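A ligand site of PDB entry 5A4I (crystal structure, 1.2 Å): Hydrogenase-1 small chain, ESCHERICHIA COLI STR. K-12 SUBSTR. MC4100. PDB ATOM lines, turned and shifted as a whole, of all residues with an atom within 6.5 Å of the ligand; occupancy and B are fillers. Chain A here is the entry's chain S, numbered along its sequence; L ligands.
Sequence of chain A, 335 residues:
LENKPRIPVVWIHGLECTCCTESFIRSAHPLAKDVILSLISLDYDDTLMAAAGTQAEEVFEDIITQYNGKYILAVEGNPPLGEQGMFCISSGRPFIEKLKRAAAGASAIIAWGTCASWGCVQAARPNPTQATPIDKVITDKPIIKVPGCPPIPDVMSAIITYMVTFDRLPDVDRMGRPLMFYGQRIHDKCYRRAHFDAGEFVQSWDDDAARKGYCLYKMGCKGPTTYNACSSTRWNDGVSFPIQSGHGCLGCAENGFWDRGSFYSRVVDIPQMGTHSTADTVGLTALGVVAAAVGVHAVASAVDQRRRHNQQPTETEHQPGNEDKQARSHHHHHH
FE3 of the ligand is bound by ND1 of His 187, 2.1 Å away.
SG of Cys 215 is bound to FE1 of the ligand, 2.3 Å away.
SG of Cys 190 is bound to FE4 of the ligand, at 2.3 Å.
An iron atom (FE2) of the ligand is bound by the side-chain sulfur (SG) of Cys 221, 2.3 Å away.
The backbone NH (N) of Leu 216 sits close to a sulfur (S3) of the ligand (3.5 Å).
S2 of the ligand lies close to N of Arg 193 (3.6 Å).
Residues that only touch the ligand: Arg 192 (3.7 Å), Tyr 217 (3.7 Å), Ile 243 (3.7 Å), Gly 223 (3.8 Å), Phe 196 (3.9 Å) and Pro 224 (3.9 Å).
Hydrophobic or aromatic side chains that line the ligand: His 187, Phe 196, Tyr 217, Pro 224 and Ile 243.
12 residues have an atom within 4 Å of the ligand: His 187, Cys 190, Arg 192, Arg 193, Phe 196, Cys 215, Leu 216, Tyr 217, Cys 221, Gly 223, Pro 224 and Ile 243.
O of His 187 sits at hydrogen-bond distance from NH1 of Arg 193 (3.1 Å).
The backbone NH (N) of Tyr 217 sits close to the side-chain sulfur (SG) of Cys 215, at 3.3 Å.
SG of Cys 190 sits close to N of Arg 192.
The side-chain sulfur (SG) of Cys 221 lies close to the backbone NH (N) of Gly 223.
The backbone NH of Cys 249 sits close to the side-chain sulfur of Cys 221, at 3.4 Å.
The guanidinium group (NH1) of Arg 193 is in salt-bridge range of the side-chain carboxylate (OD1) of Asp 188 (3.2 Å).
NH2 of Arg 192 sits at hydrogen-bond distance from O of Ile 243 (3.1 Å).
NH2 of Arg 192 lies within hydrogen-bond range of OH of Tyr 191, at 3.1 Å.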
ATOM      1  N   ILE A 186     -12.866  18.549  -4.772  1.00  0.00           N
ATOM      2  CA  ILE A 186     -13.865  17.511  -4.511  1.00  0.00           C
ATOM      3  C   ILE A 186     -13.239  16.365  -3.727  1.00  0.00           C
ATOM      4  O   ILE A 186     -13.786  15.882  -2.728  1.00  0.00           O
ATOM      5  CB  ILE A 186     -14.509  16.984  -5.849  1.00  0.00           C
ATOM      6  CG1 ILE A 186     -15.351  18.060  -6.545  1.00  0.00           C
ATOM      7  CG2 ILE A 186     -15.295  15.720  -5.605  1.00  0.00           C
ATOM      8  CD1 ILE A 186     -16.583  18.454  -5.842  1.00  0.00           C
ATOM      9  N   HIS A 187     -12.099  15.911  -4.205  1.00  0.00           N
ATOM     10  CA  HIS A 187     -11.367  14.753  -3.623  1.00  0.00           C
ATOM     11  C   HIS A 187     -10.832  15.003  -2.229  1.00  0.00           C
ATOM     12  O   HIS A 187     -10.532  14.028  -1.556  1.00  0.00           O
ATOM     13  CB  HIS A 187     -10.259  14.443  -4.646  1.00  0.00           C
ATOM     14  CG  HIS A 187      -9.298  13.344  -4.359  1.00  0.00           C
ATOM     15  ND1 HIS A 187      -9.593  12.017  -4.501  1.00  0.00           N
ATOM     16  CD2 HIS A 187      -7.955  13.391  -4.124  1.00  0.00           C
ATOM     17  CE1 HIS A 187      -8.520  11.287  -4.298  1.00  0.00           C
ATOM     18  NE2 HIS A 187      -7.498  12.097  -4.055  1.00  0.00           N
ATOM     19  N   ASP A 188     -10.683  16.269  -1.815  1.00  0.00           N
ATOM     20  CA  ASP A 188     -10.255  16.581  -0.477  1.00  0.00           C
ATOM     21  C   ASP A 188     -11.352  16.599   0.557  1.00  0.00           C
ATOM     22  O   ASP A 188     -11.046  16.728   1.734  1.00  0.00           O
ATOM     23  CB  ASP A 188      -9.409  17.823  -0.535  1.00  0.00           C
ATOM     24  CG  ASP A 188      -8.037  17.528  -1.293  1.00  0.00           C
ATOM     25  OD1 ASP A 188      -7.527  16.348  -1.378  1.00  0.00           O
ATOM     26  OD2 ASP A 188      -7.442  18.444  -1.776  1.00  0.00           O
ATOM     27  N   CYS A 190     -14.113  14.120  -0.105  1.00  0.00           N
ATOM     28  CA  CYS A 190     -14.930  13.055  -0.642  1.00  0.00           C
ATOM     29  C   CYS A 190     -15.037  11.926   0.359  1.00  0.00           C
ATOM     30  O   CYS A 190     -14.041  11.377   0.859  1.00  0.00           O
ATOM     31  CB  CYS A 190     -14.327  12.503  -1.906  1.00  0.00           C
ATOM     32  SG  CYS A 190     -15.342  11.184  -2.711  1.00  0.00           S
ATOM     33  N   TYR A 191     -16.274  11.475   0.580  1.00  0.00           N
ATOM     34  CA  TYR A 191     -16.544  10.386   1.535  1.00  0.00           C
ATOM     35  C   TYR A 191     -16.055   9.030   1.063  1.00  0.00           C
ATOM     36  O   TYR A 191     -16.027   8.134   1.875  1.00  0.00           O
ATOM     37  CB  TYR A 191     -18.053  10.360   1.911  1.00  0.00           C
ATOM     38  CG  TYR A 191     -18.927   9.607   0.940  1.00  0.00           C
ATOM     39  CD1 TYR A 191     -18.996   9.922  -0.436  1.00  0.00           C
ATOM     40  CD2 TYR A 191     -19.775   8.580   1.382  1.00  0.00           C
ATOM     41  CE1 TYR A 191     -19.830   9.222  -1.287  1.00  0.00           C
ATOM     42  CE2 TYR A 191     -20.570   7.866   0.511  1.00  0.00           C
ATOM     43  CZ  TYR A 191     -20.571   8.167  -0.831  1.00  0.00           C
ATOM     44  OH  TYR A 191     -21.301   7.425  -1.735  1.00  0.00           O
ATOM     45  N   ARG A 192     -15.598   8.893  -0.193  1.00  0.00           N
ATOM     46  CA  ARG A 192     -14.989   7.652  -0.646  1.00  0.00           C
ATOM     47  C   ARG A 192     -13.461   7.684  -0.553  1.00  0.00           C
ATOM     48  O   ARG A 192     -12.812   6.700  -0.969  1.00  0.00           O
ATOM     49  CB  ARG A 192     -15.455   7.260  -2.049  1.00  0.00           C
ATOM     50  CG  ARG A 192     -16.962   7.063  -2.099  1.00  0.00           C
ATOM     51  CD  ARG A 192     -17.439   6.543  -3.452  1.00  0.00           C
ATOM     52  NE  ARG A 192     -18.886   6.428  -3.507  1.00  0.00           N
ATOM     53  CZ  ARG A 192     -19.581   5.627  -4.298  1.00  0.00           C
ATOM     54  NH1 ARG A 192     -18.989   4.820  -5.161  1.00  0.00           N
ATOM     55  NH2 ARG A 192     -20.913   5.657  -4.244  1.00  0.00           N
ATOM     56  N   ARG A 193     -12.900   8.718   0.046  1.00  0.00           N
ATOM     57  CA  ARG A 193     -11.441   8.838   0.072  1.00  0.00           C
ATOM     58  C   ARG A 193     -10.789   7.714   0.874  1.00  0.00           C
ATOM     59  O   ARG A 193      -9.697   7.286   0.492  1.00  0.00           O
ATOM     60  CB  ARG A 193     -11.057  10.154   0.644  1.00  0.00           C
ATOM     61  CG  ARG A 193      -9.605  10.501   0.623  1.00  0.00           C
ATOM     62  CD  ARG A 193      -9.011  10.617  -0.785  1.00  0.00           C
ATOM     63  NE  ARG A 193      -7.612  10.895  -0.548  1.00  0.00           N
ATOM     64  CZ  ARG A 193      -7.042  12.070  -0.513  1.00  0.00           C
ATOM     65  NH1 ARG A 193      -7.679  13.179  -0.882  1.00  0.00           N
ATOM     66  NH2 ARG A 193      -5.792  12.132  -0.137  1.00  0.00           N
ATOM     67  N   ALA A 194     -11.433   7.173   1.891  1.00  0.00           N
ATOM     68  CA  ALA A 194     -10.915   5.991   2.593  1.00  0.00           C
ATOM     69  C   ALA A 194     -10.596   4.890   1.601  1.00  0.00           C
ATOM     70  O   ALA A 194      -9.590   4.171   1.738  1.00  0.00           O
ATOM     71  CB  ALA A 194     -11.916   5.504   3.603  1.00  0.00           C
ATOM     72  N   HIS A 195     -11.494   4.681   0.640  1.00  0.00           N
ATOM     73  CA  HIS A 195     -11.303   3.606  -0.337  1.00  0.00           C
ATOM     74  C   HIS A 195     -10.157   3.929  -1.302  1.00  0.00           C
ATOM     75  O   HIS A 195      -9.310   3.056  -1.590  1.00  0.00           O
ATOM     76  CB  HIS A 195     -12.574   3.326  -1.069  1.00  0.00           C
ATOM     77  CG  HIS A 195     -13.698   2.953  -0.177  1.00  0.00           C
ATOM     78  ND1 HIS A 195     -13.618   1.901   0.694  1.00  0.00           N
ATOM     79  CD2 HIS A 195     -14.935   3.481   0.000  1.00  0.00           C
ATOM     80  CE1 HIS A 195     -14.767   1.779   1.347  1.00  0.00           C
ATOM     81  NE2 HIS A 195     -15.578   2.719   0.931  1.00  0.00           N
ATOM     82  N   PHE A 196     -10.068   5.182  -1.766  1.00  0.00           N
ATOM     83  CA  PHE A 196      -8.931   5.615  -2.580  1.00  0.00           C
ATOM     84  C   PHE A 196      -7.631   5.292  -1.841  1.00  0.00           C
ATOM     85  O   PHE A 196      -6.702   4.722  -2.418  1.00  0.00           O
ATOM     86  CB  PHE A 196      -9.032   7.083  -2.852  1.00  0.00           C
ATOM     87  CG  PHE A 196      -7.900   7.665  -3.661  1.00  0.00           C
ATOM     88  CD1 PHE A 196      -7.948   7.686  -5.026  1.00  0.00           C
ATOM     89  CD2 PHE A 196      -6.806   8.223  -3.019  1.00  0.00           C
ATOM     90  CE1 PHE A 196      -6.907   8.242  -5.776  1.00  0.00           C
ATOM     91  CE2 PHE A 196      -5.768   8.814  -3.740  1.00  0.00           C
ATOM     92  CZ  PHE A 196      -5.823   8.807  -5.113  1.00  0.00           C
ATOM     93  N   PHE A 201     -11.150   0.061  -5.289  1.00  0.00           N
ATOM     94  CA  PHE A 201     -11.693   0.739  -6.461  1.00  0.00           C
ATOM     95  C   PHE A 201     -12.779  -0.087  -7.138  1.00  0.00           C
ATOM     96  O   PHE A 201     -12.643  -1.297  -7.336  1.00  0.00           O
ATOM     97  CB  PHE A 201     -10.588   0.972  -7.484  1.00  0.00           C
ATOM     98  CG  PHE A 201      -9.440   1.823  -6.991  1.00  0.00           C
ATOM     99  CD1 PHE A 201      -9.637   3.176  -6.680  1.00  0.00           C
ATOM    100  CD2 PHE A 201      -8.147   1.281  -6.773  1.00  0.00           C
ATOM    101  CE1 PHE A 201      -8.620   3.950  -6.219  1.00  0.00           C
ATOM    102  CE2 PHE A 201      -7.121   2.082  -6.377  1.00  0.00           C
ATOM    103  CZ  PHE A 201      -7.345   3.409  -6.065  1.00  0.00           C
ATOM    104  N   TYR A 214     -17.153   1.824  -3.295  1.00  0.00           N
ATOM    105  CA  TYR A 214     -15.715   2.055  -3.387  1.00  0.00           C
ATOM    106  C   TYR A 214     -15.407   3.216  -4.331  1.00  0.00           C
ATOM    107  O   TYR A 214     -16.261   3.774  -5.023  1.00  0.00           O
ATOM    108  CB  TYR A 214     -15.020   0.744  -3.850  1.00  0.00           C
ATOM    109  CG  TYR A 214     -14.826  -0.284  -2.776  1.00  0.00           C
ATOM    110  CD1 TYR A 214     -15.421  -0.208  -1.528  1.00  0.00           C
ATOM    111  CD2 TYR A 214     -14.050  -1.408  -3.061  1.00  0.00           C
ATOM    112  CE1 TYR A 214     -15.224  -1.197  -0.558  1.00  0.00           C
ATOM    113  CE2 TYR A 214     -13.874  -2.397  -2.113  1.00  0.00           C
ATOM    114  CZ  TYR A 214     -14.480  -2.290  -0.889  1.00  0.00           C
ATOM    115  OH  TYR A 214     -14.262  -3.272   0.075  1.00  0.00           O
ATOM    116  N   CYS A 215     -14.160   3.654  -4.317  1.00  0.00           N
ATOM    117  CA  CYS A 215     -13.699   4.840  -5.013  1.00  0.00           C
ATOM    118  C   CYS A 215     -13.818   4.633  -6.534  1.00  0.00           C
ATOM    119  O   CYS A 215     -13.620   3.515  -7.045  1.00  0.00           O
ATOM    120  CB  CYS A 215     -12.263   5.167  -4.595  1.00  0.00           C
ATOM    121  SG  CYS A 215     -11.402   6.398  -5.606  1.00  0.00           S
ATOM    122  N   LEU A 216     -14.104   5.708  -7.232  1.00  0.00           N
ATOM    123  CA  LEU A 216     -14.367   5.766  -8.669  1.00  0.00           C
ATOM    124  C   LEU A 216     -13.181   6.229  -9.513  1.00  0.00           C
ATOM    125  O   LEU A 216     -13.321   6.442 -10.724  1.00  0.00           O
ATOM    126  CB  LEU A 216     -15.606   6.615  -8.930  1.00  0.00           C
ATOM    127  CG  LEU A 216     -16.846   6.034  -8.266  1.00  0.00           C
ATOM    128  CD1 LEU A 216     -17.998   7.013  -8.299  1.00  0.00           C
ATOM    129  CD2 LEU A 216     -17.310   4.760  -8.885  1.00  0.00           C
ATOM    130  N   TYR A 217     -12.002   6.327  -8.896  1.00  0.00           N
ATOM    131  CA  TYR A 217     -10.787   6.801  -9.610  1.00  0.00           C
ATOM    132  C   TYR A 217     -10.498   6.008 -10.890  1.00  0.00           C
ATOM    133  O   TYR A 217     -10.205   6.583 -11.931  1.00  0.00           O
ATOM    134  CB  TYR A 217      -9.619   6.727  -8.624  1.00  0.00           C
ATOM    135  CG  TYR A 217      -8.294   6.976  -9.270  1.00  0.00           C
ATOM    136  CD1 TYR A 217      -7.905   8.240  -9.684  1.00  0.00           C
ATOM    137  CD2 TYR A 217      -7.434   5.911  -9.491  1.00  0.00           C
ATOM    138  CE1 TYR A 217      -6.669   8.465 -10.324  1.00  0.00           C
ATOM    139  CE2 TYR A 217      -6.208   6.094 -10.122  1.00  0.00           C
ATOM    140  CZ  TYR A 217      -5.792   7.382 -10.569  1.00  0.00           C
ATOM    141  OH  TYR A 217      -4.585   7.578 -11.157  1.00  0.00           O
ATOM    142  N   LYS A 218     -10.592   4.690 -10.805  1.00  0.00           N
ATOM    143  CA  LYS A 218     -10.288   3.849 -11.961  1.00  0.00           C
ATOM    144  C   LYS A 218     -11.372   3.878 -13.014  1.00  0.00           C
ATOM    145  O   LYS A 218     -11.174   3.457 -14.136  1.00  0.00           O
ATOM    146  CB  LYS A 218      -9.959   2.402 -11.570  1.00  0.00           C
ATOM    147  CG  LYS A 218      -8.673   2.285 -10.760  1.00  0.00           C
ATOM    148  CD  LYS A 218      -8.258   0.828 -10.601  1.00  0.00           C
ATOM    149  CE  LYS A 218      -6.869   0.814  -9.984  1.00  0.00           C
ATOM    150  NZ  LYS A 218      -6.367  -0.570  -9.737  1.00  0.00           N
ATOM    151  N   CYS A 221     -12.960   9.145 -12.384  1.00  0.00           N
ATOM    152  CA  CYS A 221     -13.340  10.270 -11.546  1.00  0.00           C
ATOM    153  C   CYS A 221     -12.306  11.389 -11.628  1.00  0.00           C
ATOM    154  O   CYS A 221     -11.114  11.158 -11.372  1.00  0.00           O
ATOM    155  CB  CYS A 221     -13.438   9.829 -10.072  1.00  0.00           C
ATOM    156  SG  CYS A 221     -14.051  11.127  -9.005  1.00  0.00           S
ATOM    157  N   LYS A 222     -12.751  12.626 -11.886  1.00  0.00           N
ATOM    158  CA  LYS A 222     -11.902  13.791 -11.942  1.00  0.00           C
ATOM    159  C   LYS A 222     -11.930  14.641 -10.665  1.00  0.00           C
ATOM    160  O   LYS A 222     -11.412  15.766 -10.637  1.00  0.00           O
ATOM    161  CB  LYS A 222     -12.248  14.638 -13.199  1.00  0.00           C
ATOM    162  CG  LYS A 222     -12.039  13.811 -14.516  1.00  0.00           C
ATOM    163  CD  LYS A 222     -10.695  13.063 -14.562  1.00  0.00           C
ATOM    164  CE  LYS A 222     -10.340  12.375 -15.851  1.00  0.00           C
ATOM    165  NZ  LYS A 222     -11.399  11.578 -16.467  1.00  0.00           N
ATOM    166  N   GLY A 223     -12.480  14.067  -9.606  1.00  0.00           N
ATOM    167  CA  GLY A 223     -12.454  14.712  -8.325  1.00  0.00           C
ATOM    168  C   GLY A 223     -11.103  15.246  -7.894  1.00  0.00           C
ATOM    169  O   GLY A 223     -11.026  16.319  -7.297  1.00  0.00           O
ATOM    170  N   PRO A 224     -10.027  14.471  -8.157  1.00  0.00           N
ATOM    171  CA  PRO A 224      -8.711  14.944  -7.704  1.00  0.00           C
ATOM    172  C   PRO A 224      -8.218  16.280  -8.276  1.00  0.00           C
ATOM    173  O   PRO A 224      -7.293  16.850  -7.730  1.00  0.00           O
ATOM    174  CB  PRO A 224      -7.763  13.793  -8.114  1.00  0.00           C
ATOM    175  CG  PRO A 224      -8.638  12.605  -8.035  1.00  0.00           C
ATOM    176  CD  PRO A 224      -9.942  13.062  -8.596  1.00  0.00           C
ATOM    177  N   PHE A 241     -24.681  13.604  -4.762  1.00  0.00           N
ATOM    178  CA  PHE A 241     -23.796  14.257  -5.699  1.00  0.00           C
ATOM    179  C   PHE A 241     -23.351  13.173  -6.666  1.00  0.00           C
ATOM    180  O   PHE A 241     -23.593  11.985  -6.426  1.00  0.00           O
ATOM    181  CB  PHE A 241     -22.669  15.044  -5.028  1.00  0.00           C
ATOM    182  CG  PHE A 241     -21.527  14.261  -4.419  1.00  0.00           C
ATOM    183  CD1 PHE A 241     -21.666  13.525  -3.270  1.00  0.00           C
ATOM    184  CD2 PHE A 241     -20.237  14.424  -4.955  1.00  0.00           C
ATOM    185  CE1 PHE A 241     -20.561  12.886  -2.690  1.00  0.00           C
ATOM    186  CE2 PHE A 241     -19.170  13.797  -4.386  1.00  0.00           C
ATOM    187  CZ  PHE A 241     -19.337  13.031  -3.258  1.00  0.00           C
ATOM    188  N   ILE A 243     -20.672  11.390  -7.411  1.00  0.00           N
ATOM    189  CA  ILE A 243     -19.953  10.256  -6.865  1.00  0.00           C
ATOM    190  C   ILE A 243     -20.826   9.440  -5.926  1.00  0.00           C
ATOM    191  O   ILE A 243     -20.766   8.191  -5.955  1.00  0.00           O
ATOM    192  CB  ILE A 243     -18.664  10.776  -6.174  1.00  0.00           C
ATOM    193  CG1 ILE A 243     -17.648  11.237  -7.219  1.00  0.00           C
ATOM    194  CG2 ILE A 243     -18.066   9.743  -5.231  1.00  0.00           C
ATOM    195  CD1 ILE A 243     -16.761  12.362  -6.765  1.00  0.00           C
ATOM    196  N   GLY A 248     -18.173   8.806 -11.467  1.00  0.00           N
ATOM    197  CA  GLY A 248     -17.089   9.706 -11.175  1.00  0.00           C
ATOM    198  C   GLY A 248     -17.450  11.151 -11.528  1.00  0.00           C
ATOM    199  O   GLY A 248     -18.201  11.422 -12.469  1.00  0.00           O
ATOM    200  N   CYS A 249     -16.795  12.073 -10.835  1.00  0.00           N
ATOM    201  CA  CYS A 249     -16.825  13.476 -11.241  1.00  0.00           C
ATOM    202  C   CYS A 249     -16.310  13.602 -12.695  1.00  0.00           C
ATOM    203  O   CYS A 249     -15.321  12.965 -13.076  1.00  0.00           O
ATOM    204  CB  CYS A 249     -15.954  14.260 -10.263  1.00  0.00           C
ATOM    205  SG  CYS A 249     -15.715  16.024 -10.586  1.00  0.00           S
HETATM  206 FE1  LIG L   1     -12.279   8.469  -5.321  1.00  0.00          FE
HETATM  207 FE2  LIG L   1     -13.270  10.478  -6.935  1.00  0.00          FE
HETATM  208 FE3  LIG L   1     -11.346  10.998  -5.069  1.00  0.00          FE
HETATM  209 FE4  LIG L   1     -13.860  10.445  -4.274  1.00  0.00          FE
HETATM  210  S1  LIG L   1     -13.164  12.279  -5.522  1.00  0.00           S
HETATM  211  S2  LIG L   1     -11.954   9.581  -3.357  1.00  0.00           S
HETATM  212  S3  LIG L   1     -14.488   8.851  -5.806  1.00  0.00           S
HETATM  213  S4  LIG L   1     -11.124   9.688  -6.930  1.00  0.00           S
